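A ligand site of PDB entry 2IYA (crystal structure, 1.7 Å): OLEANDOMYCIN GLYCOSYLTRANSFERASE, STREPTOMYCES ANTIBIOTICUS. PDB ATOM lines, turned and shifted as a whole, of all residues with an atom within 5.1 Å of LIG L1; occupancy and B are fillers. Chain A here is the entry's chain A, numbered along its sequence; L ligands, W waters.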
ATOM      1  N   ILE A  20      17.974 -24.201   0.016  1.00  0.00           N
ATOM      2  CA  ILE A  20      16.626 -23.750  -0.273  1.00  0.00           C
ATOM      3  C   ILE A  20      15.893 -24.839  -1.052  1.00  0.00           C
ATOM      4  O   ILE A  20      16.532 -25.677  -1.737  1.00  0.00           O
ATOM      5  CB  ILE A  20      16.601 -22.411  -1.076  1.00  0.00           C
ATOM      6  CG1 ILE A  20      17.200 -22.603  -2.486  1.00  0.00           C
ATOM      7  CG2 ILE A  20      17.336 -21.298  -0.310  1.00  0.00           C
ATOM      8  CD1 ILE A  20      16.405 -21.926  -3.590  1.00  0.00           C
ATOM      9  N   HIS A  25      19.028 -26.428  -6.640  1.00  0.00           N
ATOM     10  CA  HIS A  25      19.925 -25.976  -5.566  1.00  0.00           C
ATOM     11  C   HIS A  25      20.353 -27.144  -4.659  1.00  0.00           C
ATOM     12  O   HIS A  25      21.497 -27.207  -4.252  1.00  0.00           O
ATOM     13  CB  HIS A  25      19.274 -24.863  -4.766  1.00  0.00           C
ATOM     14  CG  HIS A  25      19.111 -23.598  -5.542  1.00  0.00           C
ATOM     15  ND1 HIS A  25      19.820 -22.447  -5.250  1.00  0.00           N
ATOM     16  CD2 HIS A  25      18.380 -23.313  -6.638  1.00  0.00           C
ATOM     17  CE1 HIS A  25      19.497 -21.500  -6.108  1.00  0.00           C
ATOM     18  NE2 HIS A  25      18.632 -22.009  -6.983  1.00  0.00           N
ATOM     19  N   TRP A  79       7.580 -20.139  -9.090  1.00  0.00           N
ATOM     20  CA  TRP A  79       8.582 -19.082  -8.979  1.00  0.00           C
ATOM     21  C   TRP A  79       8.290 -17.963  -9.976  1.00  0.00           C
ATOM     22  O   TRP A  79       7.700 -18.194 -11.053  1.00  0.00           O
ATOM     23  CB  TRP A  79       9.960 -19.659  -9.301  1.00  0.00           C
ATOM     24  CG  TRP A  79      10.448 -20.676  -8.341  1.00  0.00           C
ATOM     25  CD1 TRP A  79      10.373 -22.017  -8.472  1.00  0.00           C
ATOM     26  CD2 TRP A  79      11.141 -20.423  -7.112  1.00  0.00           C
ATOM     27  NE1 TRP A  79      10.963 -22.644  -7.395  1.00  0.00           N
ATOM     28  CE2 TRP A  79      11.439 -21.683  -6.535  1.00  0.00           C
ATOM     29  CE3 TRP A  79      11.550 -19.254  -6.449  1.00  0.00           C
ATOM     30  CZ2 TRP A  79      12.120 -21.815  -5.317  1.00  0.00           C
ATOM     31  CZ3 TRP A  79      12.223 -19.386  -5.219  1.00  0.00           C
ATOM     32  CH2 TRP A  79      12.498 -20.662  -4.676  1.00  0.00           C
ATOM     33  N   PRO A  80       8.734 -16.732  -9.639  1.00  0.00           N
ATOM     34  CA  PRO A  80       8.689 -15.677 -10.641  1.00  0.00           C
ATOM     35  C   PRO A  80       9.844 -15.896 -11.620  1.00  0.00           C
ATOM     36  O   PRO A  80      10.776 -16.647 -11.307  1.00  0.00           O
ATOM     37  CB  PRO A  80       8.957 -14.412  -9.819  1.00  0.00           C
ATOM     38  CG  PRO A  80       9.857 -14.870  -8.721  1.00  0.00           C
ATOM     39  CD  PRO A  80       9.394 -16.288  -8.394  1.00  0.00           C
ATOM     40  N   GLU A  81       9.784 -15.267 -12.785  1.00  0.00           N
ATOM     41  CA  GLU A  81      10.897 -15.323 -13.756  1.00  0.00           C
ATOM     42  C   GLU A  81      11.938 -14.227 -13.521  1.00  0.00           C
ATOM     43  O   GLU A  81      13.067 -14.330 -14.009  1.00  0.00           O
ATOM     44  CB  GLU A  81      10.380 -15.224 -15.191  1.00  0.00           C
ATOM     45  CG  GLU A  81       9.691 -16.483 -15.693  1.00  0.00           C
ATOM     46  CD  GLU A  81       9.333 -16.420 -17.175  1.00  0.00           C
ATOM     47  OE1 GLU A  81       9.905 -15.590 -17.918  1.00  0.00           O
ATOM     48  OE2 GLU A  81       8.488 -17.213 -17.615  1.00  0.00           O
ATOM     49  N   ASP A  82      11.572 -13.185 -12.786  1.00  0.00           N
ATOM     50  CA  ASP A  82      12.435 -12.007 -12.678  1.00  0.00           C
ATOM     51  C   ASP A  82      13.257 -11.974 -11.392  1.00  0.00           C
ATOM     52  O   ASP A  82      12.743 -12.291 -10.305  1.00  0.00           O
ATOM     53  CB  ASP A  82      11.612 -10.721 -12.816  1.00  0.00           C
ATOM     54  CG  ASP A  82      10.573 -10.576 -11.709  1.00  0.00           C
ATOM     55  OD1 ASP A  82       9.663 -11.434 -11.628  1.00  0.00           O
ATOM     56  OD2 ASP A  82      10.685  -9.626 -10.905  1.00  0.00           O
ATOM     57  N   GLN A  83      14.506 -11.505 -11.505  1.00  0.00           N
ATOM     58  CA  GLN A  83      15.424 -11.531 -10.381  1.00  0.00           C
ATOM     59  C   GLN A  83      14.944 -10.663  -9.220  1.00  0.00           C
ATOM     60  O   GLN A  83      15.055 -11.046  -8.055  1.00  0.00           O
ATOM     61  CB  GLN A  83      16.817 -11.079 -10.818  1.00  0.00           C
ATOM     62  CG  GLN A  83      17.845 -11.172  -9.691  1.00  0.00           C
ATOM     63  CD  GLN A  83      19.253 -10.859 -10.188  1.00  0.00           C
ATOM     64  OE1 GLN A  83      19.412 -10.342 -11.284  1.00  0.00           O
ATOM     65  NE2 GLN A  83      20.270 -11.203  -9.389  1.00  0.00           N
ATOM     66  N   ALA A  86      12.348 -12.441  -7.186  1.00  0.00           N
ATOM     67  CA  ALA A  86      12.970 -13.605  -6.540  1.00  0.00           C
ATOM     68  C   ALA A  86      13.825 -13.190  -5.334  1.00  0.00           C
ATOM     69  O   ALA A  86      13.783 -13.828  -4.285  1.00  0.00           O
ATOM     70  CB  ALA A  86      13.807 -14.357  -7.513  1.00  0.00           C
ATOM     71  N   MET A  87      14.618 -12.129  -5.499  1.00  0.00           N
ATOM     72  CA  MET A  87      15.429 -11.671  -4.389  1.00  0.00           C
ATOM     73  C   MET A  87      14.553 -11.242  -3.199  1.00  0.00           C
ATOM     74  O   MET A  87      14.884 -11.525  -2.055  1.00  0.00           O
ATOM     75  CB  MET A  87      16.368 -10.518  -4.843  1.00  0.00           C
ATOM     76  CG  MET A  87      17.557 -10.978  -5.738  1.00  0.00           C
ATOM     77  SD  MET A  87      18.827  -9.642  -6.052  1.00  0.00           S
ATOM     78  CE  MET A  87      17.739  -8.419  -6.812  1.00  0.00           C
ATOM     79  N   PHE A  90      13.552 -14.316  -1.379  1.00  0.00           N
ATOM     80  CA  PHE A  90      14.630 -14.911  -0.598  1.00  0.00           C
ATOM     81  C   PHE A  90      14.915 -14.115   0.660  1.00  0.00           C
ATOM     82  O   PHE A  90      15.345 -14.685   1.673  1.00  0.00           O
ATOM     83  CB  PHE A  90      15.898 -15.095  -1.444  1.00  0.00           C
ATOM     84  CG  PHE A  90      15.790 -16.227  -2.447  1.00  0.00           C
ATOM     85  CD1 PHE A  90      15.410 -17.508  -2.044  1.00  0.00           C
ATOM     86  CD2 PHE A  90      16.042 -16.003  -3.794  1.00  0.00           C
ATOM     87  CE1 PHE A  90      15.290 -18.537  -2.979  1.00  0.00           C
ATOM     88  CE2 PHE A  90      15.933 -17.037  -4.722  1.00  0.00           C
ATOM     89  CZ  PHE A  90      15.547 -18.294  -4.320  1.00  0.00           C
ATOM     90  N   ILE A 117      23.687 -20.373  -2.588  1.00  0.00           N
ATOM     91  CA  ILE A 117      23.689 -18.951  -2.995  1.00  0.00           C
ATOM     92  C   ILE A 117      22.499 -18.159  -2.457  1.00  0.00           C
ATOM     93  O   ILE A 117      22.615 -16.956  -2.230  1.00  0.00           O
ATOM     94  CB  ILE A 117      23.809 -18.782  -4.533  1.00  0.00           C
ATOM     95  CG1 ILE A 117      22.720 -19.578  -5.300  1.00  0.00           C
ATOM     96  CG2 ILE A 117      25.193 -19.216  -4.979  1.00  0.00           C
ATOM     97  CD1 ILE A 117      22.574 -19.180  -6.817  1.00  0.00           C
ATOM     98  N   ALA A 118      21.357 -18.827  -2.258  1.00  0.00           N
ATOM     99  CA  ALA A 118      20.146 -18.153  -1.778  1.00  0.00           C
ATOM    100  C   ALA A 118      19.879 -18.334  -0.265  1.00  0.00           C
ATOM    101  O   ALA A 118      18.825 -17.900   0.239  1.00  0.00           O
ATOM    102  CB  ALA A 118      18.955 -18.634  -2.584  1.00  0.00           C
ATOM    103  N   TRP A 120      20.589 -16.963   2.679  1.00  0.00           N
ATOM    104  CA  TRP A 120      21.122 -15.769   3.310  1.00  0.00           C
ATOM    105  C   TRP A 120      21.226 -15.802   4.850  1.00  0.00           C
ATOM    106  O   TRP A 120      22.006 -15.031   5.399  1.00  0.00           O
ATOM    107  CB  TRP A 120      20.379 -14.514   2.819  1.00  0.00           C
ATOM    108  CG  TRP A 120      20.424 -14.356   1.289  1.00  0.00           C
ATOM    109  CD1 TRP A 120      21.299 -14.966   0.423  1.00  0.00           C
ATOM    110  CD2 TRP A 120      19.608 -13.488   0.487  1.00  0.00           C
ATOM    111  NE1 TRP A 120      21.032 -14.568  -0.885  1.00  0.00           N
ATOM    112  CE2 TRP A 120      19.996 -13.654  -0.862  1.00  0.00           C
ATOM    113  CE3 TRP A 120      18.551 -12.612   0.778  1.00  0.00           C
ATOM    114  CZ2 TRP A 120      19.395 -12.965  -1.916  1.00  0.00           C
ATOM    115  CZ3 TRP A 120      17.940 -11.920  -0.274  1.00  0.00           C
ATOM    116  CH2 TRP A 120      18.370 -12.104  -1.603  1.00  0.00           C
ATOM    117  N   THR A 139      25.498 -22.526  -9.790  1.00  0.00           N
ATOM    118  CA  THR A 139      25.521 -21.849 -11.099  1.00  0.00           C
ATOM    119  C   THR A 139      26.766 -20.975 -11.256  1.00  0.00           C
ATOM    120  O   THR A 139      27.650 -20.982 -10.387  1.00  0.00           O
ATOM    121  CB  THR A 139      24.205 -21.064 -11.376  1.00  0.00           C
ATOM    122  OG1 THR A 139      24.143 -20.693 -12.776  1.00  0.00           O
ATOM    123  CG2 THR A 139      24.076 -19.834 -10.454  1.00  0.00           C
ATOM    124  N   PHE A 140      26.848 -20.245 -12.365  1.00  0.00           N
ATOM    125  CA  PHE A 140      28.005 -19.385 -12.566  1.00  0.00           C
ATOM    126  C   PHE A 140      28.062 -18.283 -11.480  1.00  0.00           C
ATOM    127  O   PHE A 140      27.051 -17.933 -10.883  1.00  0.00           O
ATOM    128  CB  PHE A 140      28.060 -18.831 -13.975  1.00  0.00           C
ATOM    129  CG  PHE A 140      26.865 -18.022 -14.390  1.00  0.00           C
ATOM    130  CD1 PHE A 140      25.882 -18.582 -15.221  1.00  0.00           C
ATOM    131  CD2 PHE A 140      26.743 -16.679 -14.017  1.00  0.00           C
ATOM    132  CE1 PHE A 140      24.791 -17.815 -15.644  1.00  0.00           C
ATOM    133  CE2 PHE A 140      25.668 -15.895 -14.436  1.00  0.00           C
ATOM    134  CZ  PHE A 140      24.682 -16.480 -15.254  1.00  0.00           C
ATOM    135  N   VAL A 141      29.273 -17.799 -11.230  1.00  0.00           N
ATOM    136  CA  VAL A 141      29.528 -16.803 -10.177  1.00  0.00           C
ATOM    137  C   VAL A 141      29.849 -15.431 -10.796  1.00  0.00           C
ATOM    138  O   VAL A 141      29.929 -15.284 -12.027  1.00  0.00           O
ATOM    139  CB  VAL A 141      30.700 -17.272  -9.261  1.00  0.00           C
ATOM    140  CG1 VAL A 141      30.311 -18.561  -8.518  1.00  0.00           C
ATOM    141  CG2 VAL A 141      32.003 -17.449 -10.056  1.00  0.00           C
ATOM    142  N   ALA A 142      29.979 -14.430  -9.926  1.00  0.00           N
ATOM    143  CA  ALA A 142      30.219 -13.067 -10.387  1.00  0.00           C
ATOM    144  C   ALA A 142      31.623 -13.003 -10.957  1.00  0.00           C
ATOM    145  O   ALA A 142      32.593 -13.368 -10.295  1.00  0.00           O
ATOM    146  CB  ALA A 142      30.052 -12.105  -9.251  1.00  0.00           C
ATOM    147  N   PHE A 146      30.481  -8.232 -13.584  1.00  0.00           N
ATOM    148  CA  PHE A 146      29.162  -8.884 -13.438  1.00  0.00           C
ATOM    149  C   PHE A 146      28.010  -7.907 -13.206  1.00  0.00           C
ATOM    150  O   PHE A 146      26.964  -7.989 -13.857  1.00  0.00           O
ATOM    151  CB  PHE A 146      29.208  -9.906 -12.286  1.00  0.00           C
ATOM    152  CG  PHE A 146      27.894 -10.617 -12.054  1.00  0.00           C
ATOM    153  CD1 PHE A 146      27.489 -11.649 -12.895  1.00  0.00           C
ATOM    154  CD2 PHE A 146      27.076 -10.254 -11.002  1.00  0.00           C
ATOM    155  CE1 PHE A 146      26.279 -12.314 -12.673  1.00  0.00           C
ATOM    156  CE2 PHE A 146      25.856 -10.916 -10.778  1.00  0.00           C
ATOM    157  CZ  PHE A 146      25.462 -11.938 -11.627  1.00  0.00           C
ATOM    158  N   VAL A 150      24.374  -7.581 -15.095  1.00  0.00           N
ATOM    159  CA  VAL A 150      23.197  -7.952 -14.310  1.00  0.00           C
ATOM    160  C   VAL A 150      22.902  -6.823 -13.312  1.00  0.00           C
ATOM    161  O   VAL A 150      23.122  -6.967 -12.115  1.00  0.00           O
ATOM    162  CB  VAL A 150      23.396  -9.322 -13.586  1.00  0.00           C
ATOM    163  CG1 VAL A 150      22.124  -9.748 -12.881  1.00  0.00           C
ATOM    164  CG2 VAL A 150      23.815 -10.412 -14.589  1.00  0.00           C
ATOM    165  N   VAL A 153      21.553  -6.277  -9.351  1.00  0.00           N
ATOM    166  CA  VAL A 153      22.317  -6.443  -8.102  1.00  0.00           C
ATOM    167  C   VAL A 153      22.945  -5.150  -7.580  1.00  0.00           C
ATOM    168  O   VAL A 153      23.473  -5.129  -6.457  1.00  0.00           O
ATOM    169  CB  VAL A 153      23.408  -7.551  -8.231  1.00  0.00           C
ATOM    170  CG1 VAL A 153      22.788  -8.910  -8.649  1.00  0.00           C
ATOM    171  CG2 VAL A 153      24.569  -7.111  -9.203  1.00  0.00           C
ATOM    172  N   LEU A 207      25.339  -9.885  -1.663  1.00  0.00           N
ATOM    173  CA  LEU A 207      24.622 -10.649  -2.676  1.00  0.00           C
ATOM    174  C   LEU A 207      25.548 -11.420  -3.605  1.00  0.00           C
ATOM    175  O   LEU A 207      25.246 -12.568  -3.967  1.00  0.00           O
ATOM    176  CB  LEU A 207      23.687  -9.756  -3.474  1.00  0.00           C
ATOM    177  CG  LEU A 207      22.555  -9.087  -2.688  1.00  0.00           C
ATOM    178  CD1 LEU A 207      21.907  -8.007  -3.540  1.00  0.00           C
ATOM    179  CD2 LEU A 207      21.533 -10.165  -2.217  1.00  0.00           C
ATOM    180  N   ILE A 208      26.669 -10.814  -4.014  1.00  0.00           N
ATOM    181  CA  ILE A 208      27.432 -11.364  -5.153  1.00  0.00           C
ATOM    182  C   ILE A 208      28.902 -11.739  -4.921  1.00  0.00           C
ATOM    183  O   ILE A 208      29.553 -12.262  -5.843  1.00  0.00           O
ATOM    184  CB  ILE A 208      27.339 -10.440  -6.405  1.00  0.00           C
ATOM    185  CG1 ILE A 208      28.185  -9.151  -6.214  1.00  0.00           C
ATOM    186  CG2 ILE A 208      25.859 -10.111  -6.769  1.00  0.00           C
ATOM    187  CD1 ILE A 208      28.307  -8.275  -7.493  1.00  0.00           C
ATOM    188  N   ALA A 265      11.547 -26.363 -12.299  1.00  0.00           N
ATOM    189  CA  ALA A 265      10.783 -25.159 -11.952  1.00  0.00           C
ATOM    190  C   ALA A 265       9.911 -24.604 -13.075  1.00  0.00           C
ATOM    191  O   ALA A 265       8.694 -24.452 -12.887  1.00  0.00           O
ATOM    192  CB  ALA A 265      11.711 -24.058 -11.389  1.00  0.00           C
ATOM    193  N   PHE A 266      10.505 -24.311 -14.204  1.00  0.00           N
ATOM    194  CA  PHE A 266       9.785 -23.528 -15.230  1.00  0.00           C
ATOM    195  C   PHE A 266       9.282 -24.451 -16.340  1.00  0.00           C
ATOM    196  O   PHE A 266       9.698 -24.347 -17.485  1.00  0.00           O
ATOM    197  CB  PHE A 266      10.703 -22.445 -15.790  1.00  0.00           C
ATOM    198  CG  PHE A 266      11.066 -21.408 -14.771  1.00  0.00           C
ATOM    199  CD1 PHE A 266      10.125 -20.472 -14.360  1.00  0.00           C
ATOM    200  CD2 PHE A 266      12.334 -21.400 -14.178  1.00  0.00           C
ATOM    201  CE1 PHE A 266      10.451 -19.497 -13.388  1.00  0.00           C
ATOM    202  CE2 PHE A 266      12.660 -20.452 -13.226  1.00  0.00           C
ATOM    203  CZ  PHE A 266      11.725 -19.512 -12.836  1.00  0.00           C
ATOM    204  N   ILE A 350      14.681 -18.585 -18.585  1.00  0.00           N
ATOM    205  CA  ILE A 350      15.071 -17.337 -17.947  1.00  0.00           C
ATOM    206  C   ILE A 350      16.475 -16.917 -18.396  1.00  0.00           C
ATOM    207  O   ILE A 350      17.200 -17.716 -18.974  1.00  0.00           O
ATOM    208  CB  ILE A 350      14.957 -17.416 -16.390  1.00  0.00           C
ATOM    209  CG1 ILE A 350      15.909 -18.483 -15.835  1.00  0.00           C
ATOM    210  CG2 ILE A 350      13.486 -17.682 -15.986  1.00  0.00           C
ATOM    211  CD1 ILE A 350      16.064 -18.476 -14.300  1.00  0.00           C
ATOM    212  N   ALA A 351      16.843 -15.662 -18.136  1.00  0.00           N
ATOM    213  CA  ALA A 351      18.139 -15.138 -18.566  1.00  0.00           C
ATOM    214  C   ALA A 351      19.349 -15.988 -18.178  1.00  0.00           C
ATOM    215  O   ALA A 351      20.273 -16.151 -18.987  1.00  0.00           O
ATOM    216  CB  ALA A 351      18.345 -13.679 -18.085  1.00  0.00           C
ATOM    217  N   GLU A 352      19.368 -16.529 -16.968  1.00  0.00           N
ATOM    218  CA  GLU A 352      20.481 -17.410 -16.555  1.00  0.00           C
ATOM    219  C   GLU A 352      20.633 -18.542 -17.575  1.00  0.00           C
ATOM    220  O   GLU A 352      21.734 -18.847 -18.011  1.00  0.00           O
ATOM    221  CB  GLU A 352      20.216 -18.020 -15.176  1.00  0.00           C
ATOM    222  CG  GLU A 352      21.342 -18.955 -14.740  1.00  0.00           C
ATOM    223  CD  GLU A 352      20.834 -20.189 -14.025  1.00  0.00           C
ATOM    224  OE1 GLU A 352      19.603 -20.330 -13.859  1.00  0.00           O
ATOM    225  OE2 GLU A 352      21.672 -21.024 -13.620  1.00  0.00           O
ATOM    226  N   MET A 355      22.100 -17.496 -20.892  1.00  0.00           N
ATOM    227  CA  MET A 355      23.572 -17.372 -20.769  1.00  0.00           C
ATOM    228  C   MET A 355      24.241 -18.773 -20.859  1.00  0.00           C
ATOM    229  O   MET A 355      25.251 -18.939 -21.565  1.00  0.00           O
ATOM    230  CB  MET A 355      23.947 -16.606 -19.502  1.00  0.00           C
ATOM    231  CG  MET A 355      23.486 -15.134 -19.546  1.00  0.00           C
ATOM    232  SD  MET A 355      24.061 -14.082 -18.170  1.00  0.00           S
ATOM    233  CE  MET A 355      23.369 -12.497 -18.654  1.00  0.00           C
HETATM  234  C1  LIG L   1      21.943 -13.413  -6.043  1.00  0.00           C
HETATM  235  C2  LIG L   1      22.836 -13.592  -7.289  1.00  0.00           C
HETATM  236  C3  LIG L   1      24.352 -13.940  -7.162  1.00  0.00           C
HETATM  237  C4  LIG L   1      24.968 -14.103  -8.575  1.00  0.00           C
HETATM  238  O1  LIG L   1      24.340 -15.231  -9.181  1.00  0.00           O
HETATM  239  C5  LIG L   1      22.549 -16.307 -10.588  1.00  0.00           C
HETATM  240  C6  LIG L   1      21.044 -15.960 -10.388  1.00  0.00           C
HETATM  241  C7  LIG L   1      20.180 -17.139  -9.814  1.00  0.00           C
HETATM  242  C8  LIG L   1      18.734 -16.708  -9.403  1.00  0.00           C
HETATM  243  C9  LIG L   1      18.650 -15.523  -8.375  1.00  0.00           C
HETATM  244  C10 LIG L   1      19.142 -16.082  -7.016  1.00  0.00           C
HETATM  245  C11 LIG L   1      19.958 -15.231  -6.030  1.00  0.00           C
HETATM  246  C12 LIG L   1      20.513 -13.857  -6.418  1.00  0.00           C
HETATM  247  O2  LIG L   1      19.727 -12.947  -7.136  1.00  0.00           O
HETATM  248  C13 LIG L   1      23.377 -15.073 -10.189  1.00  0.00           C
HETATM  249  O3  LIG L   1      23.098 -13.806 -10.734  1.00  0.00           O
HETATM  250  O4  LIG L   1      20.475 -15.477 -11.590  1.00  0.00           O
HETATM  251  O5  LIG L   1      18.109 -17.827  -8.770  1.00  0.00           O
HETATM  252  C14 LIG L   1      21.952 -12.035  -5.368  1.00  0.00           C
HETATM  253  C15 LIG L   1      19.365 -15.239  -4.614  1.00  0.00           C
HETATM  254  C16 LIG L   1      24.618 -15.217  -6.341  1.00  0.00           C
HETATM  255  O6  LIG L   1      22.607 -12.518  -8.194  1.00  0.00           O
HETATM  256  C17 LIG L   1      26.489 -14.332  -8.600  1.00  0.00           C
HETATM  257  C18 LIG L   1      22.982 -16.740 -12.001  1.00  0.00           C
HETATM  258  C19 LIG L   1      17.243 -14.912  -8.217  1.00  0.00           C
HETATM  259  C20 LIG L   1      17.033 -18.356  -9.535  1.00  0.00           C
HETATM  260  C21 LIG L   1      16.720 -19.742  -8.953  1.00  0.00           C
HETATM  261  C22 LIG L   1      15.432 -20.322  -9.576  1.00  0.00           C
HETATM  262  C23 LIG L   1      14.275 -19.307  -9.543  1.00  0.00           C
HETATM  263  C24 LIG L   1      14.745 -17.996 -10.184  1.00  0.00           C
HETATM  264  O7  LIG L   1      15.890 -17.512  -9.487  1.00  0.00           O
HETATM  265  N1  LIG L   1      15.098 -21.639  -9.021  1.00  0.00           N
HETATM  266  C25 LIG L   1      13.700 -16.881 -10.092  1.00  0.00           C
HETATM  267  O8  LIG L   1      17.800 -20.634  -9.178  1.00  0.00           O
HETATM  268  C26 LIG L   1      14.013 -22.315  -9.759  1.00  0.00           C
HETATM  269  C27 LIG L   1      19.912 -14.172 -11.622  1.00  0.00           C
HETATM  270  C28 LIG L   1      20.393 -13.489 -12.923  1.00  0.00           C
HETATM  271  C29 LIG L   1      19.744 -14.125 -14.192  1.00  0.00           C
HETATM  272  C30 LIG L   1      18.205 -14.209 -14.003  1.00  0.00           C
HETATM  273  C31 LIG L   1      17.864 -14.858 -12.637  1.00  0.00           C
HETATM  274  O9  LIG L   1      18.490 -14.198 -11.538  1.00  0.00           O
HETATM  275  O10 LIG L   1      20.045 -13.375 -15.379  1.00  0.00           O
HETATM  276  O11 LIG L   1      17.642 -15.033 -15.017  1.00  0.00           O
HETATM  277  O12 LIG L   1      20.578 -15.883  -4.935  1.00  0.00           O
HETATM  278  C32 LIG L   1      21.406 -13.551 -15.789  1.00  0.00           C
HETATM  279  C33 LIG L   1      14.992 -21.769  -7.558  1.00  0.00           C
HETATM  280  C34 LIG L   1      16.355 -14.873 -12.345  1.00  0.00           C
HETATM  281  C35 LIG L   1      20.220 -18.368 -10.755  1.00  0.00           C
HETATM  282  N1  LG2 L   2      15.437 -33.396 -12.595  1.00  0.00           N
HETATM  283  C1  LG2 L   2      15.102 -34.729 -12.397  1.00  0.00           C
HETATM  284  N2  LG2 L   2      13.991 -35.248 -13.046  1.00  0.00           N
HETATM  285  C2  LG2 L   2      13.237 -34.471 -13.899  1.00  0.00           C
HETATM  286  C3  LG2 L   2      13.572 -33.123 -14.113  1.00  0.00           C
HETATM  287  C4  LG2 L   2      14.691 -32.618 -13.459  1.00  0.00           C
HETATM  288  O1  LG2 L   2      15.741 -35.450 -11.647  1.00  0.00           O
HETATM  289  O2  LG2 L   2      12.266 -34.986 -14.450  1.00  0.00           O
HETATM  290  C5  LG2 L   2      16.626 -32.860 -11.898  1.00  0.00           C
HETATM  291  C6  LG2 L   2      17.837 -32.774 -12.826  1.00  0.00           C
HETATM  292  O3  LG2 L   2      18.506 -34.015 -12.905  1.00  0.00           O
HETATM  293  C7  LG2 L   2      18.658 -31.646 -12.206  1.00  0.00           C
HETATM  294  C8  LG2 L   2      17.593 -30.766 -11.540  1.00  0.00           C
HETATM  295  O4  LG2 L   2      16.390 -31.536 -11.450  1.00  0.00           O
HETATM  296  O5  LG2 L   2      19.536 -32.115 -11.193  1.00  0.00           O
HETATM  297  C9  LG2 L   2      17.240 -29.481 -12.292  1.00  0.00           C
HETATM  298  O6  LG2 L   2      18.260 -28.539 -12.030  1.00  0.00           O
HETATM  299  P1  LG2 L   2      18.672 -27.442 -13.107  1.00  0.00           P
HETATM  300  O7  LG2 L   2      19.844 -26.751 -12.558  1.00  0.00           O
HETATM  301  O8  LG2 L   2      18.917 -28.007 -14.462  1.00  0.00           O
HETATM  302  O9  LG2 L   2      17.385 -26.560 -13.451  1.00  0.00           O
HETATM  303  P2  LG2 L   2      16.352 -25.803 -12.512  1.00  0.00           P
HETATM  304  O10 LG2 L   2      15.419 -26.825 -11.993  1.00  0.00           O
HETATM  305  O11 LG2 L   2      15.719 -24.821 -13.377  1.00  0.00           O
HETATM  306  O12 LG2 L   2      17.112 -25.164 -11.408  1.00  0.00           O
HETATM  307  O   HOH W   1      18.090 -21.209 -11.747  1.00  0.00           O
HETATM  308  O   HOH W   2      27.010 -14.731  -3.847  1.00  0.00           O
HETATM  309  O   HOH W   3      15.260 -13.843 -15.544  1.00  0.00           O
HETATM  310  O   HOH W   4      23.250 -14.197  -3.059  1.00  0.00           O
HETATM  311  O   HOH W   5      19.118 -10.867 -15.944  1.00  0.00           O
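Water W1 bridges O8 of LIG L1 and OE1 of Glu 352.
Water W3 bridges an oxygen (O11) of LIG L1 (2.7 Å) and the backbone carbonyl oxygen (O) of Glu 81 (2.7 Å).
Water W4 lies within hydrogen-bond range of O of Leu 207, O of Ile 117 and NE1 of Trp 120.
SD of Met 87 sits close to O2 of LIG L1 (3.6 Å).
Merely in contact with LIG L1: Trp 79 (3.6 Å), Pro 80 (3.2 Å), Glu 81 (3.7 Å), Ala 86 (3.6 Å), Phe 90 (3.5 Å), Ile 117 (3.6 Å), Ala 118 (3.9 Å), Trp 120 (3.5 Å), Thr 139 (3.6 Å), Phe 140 (3.7 Å), Ala 142 (3.7 Å), Phe 146 (3.1 Å), Val 153 (3.6 Å), Leu 207 (3.4 Å), Ala 265 (3.3 Å), Ile 350 (3.8 Å) and Met 355 (3.6 Å).
Hydrophobic or aromatic side chains that line LIG L1: His 25, Trp 79, Ala 86, Met 87, Phe 90, Ala 118, Trp 120, Phe 140, Phe 146, Val 153, Leu 207, Ala 265, Ile 350, Ala 351 and Met 355.
Of the 28 residues printed, 22 come within 4 Å of LIG L1.
Along chain A the residues within 4 Å of LIG L1 span positions 25 to 355.
An oxygen (O11) of LIG L1 sits at hydrogen-bond distance from the backbone NH of Ala 351, at 3.3 Å.
The backbone NH of Glu 352 sits at hydrogen-bond distance from an oxygen (O11) of LIG L1 (3.0 Å).
The side-chain amide nitrogen (NE2) of Gln 83 lies within hydrogen-bond range of an oxygen (O2) of LIG L1 (2.9 Å).
A ring nitrogen (NE2) of His 25 is in hydrogen-bond range of an oxygen (O8) of LIG L1.
The side-chain carboxylate (OE2) of Glu 352 sits at hydrogen-bond distance from the side-chain hydroxyl (OG1) of Thr 139, 2.6 Å away.
NE1 of Trp 120 lies within hydrogen-bond range of O of Ile 117 (3.2 Å).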
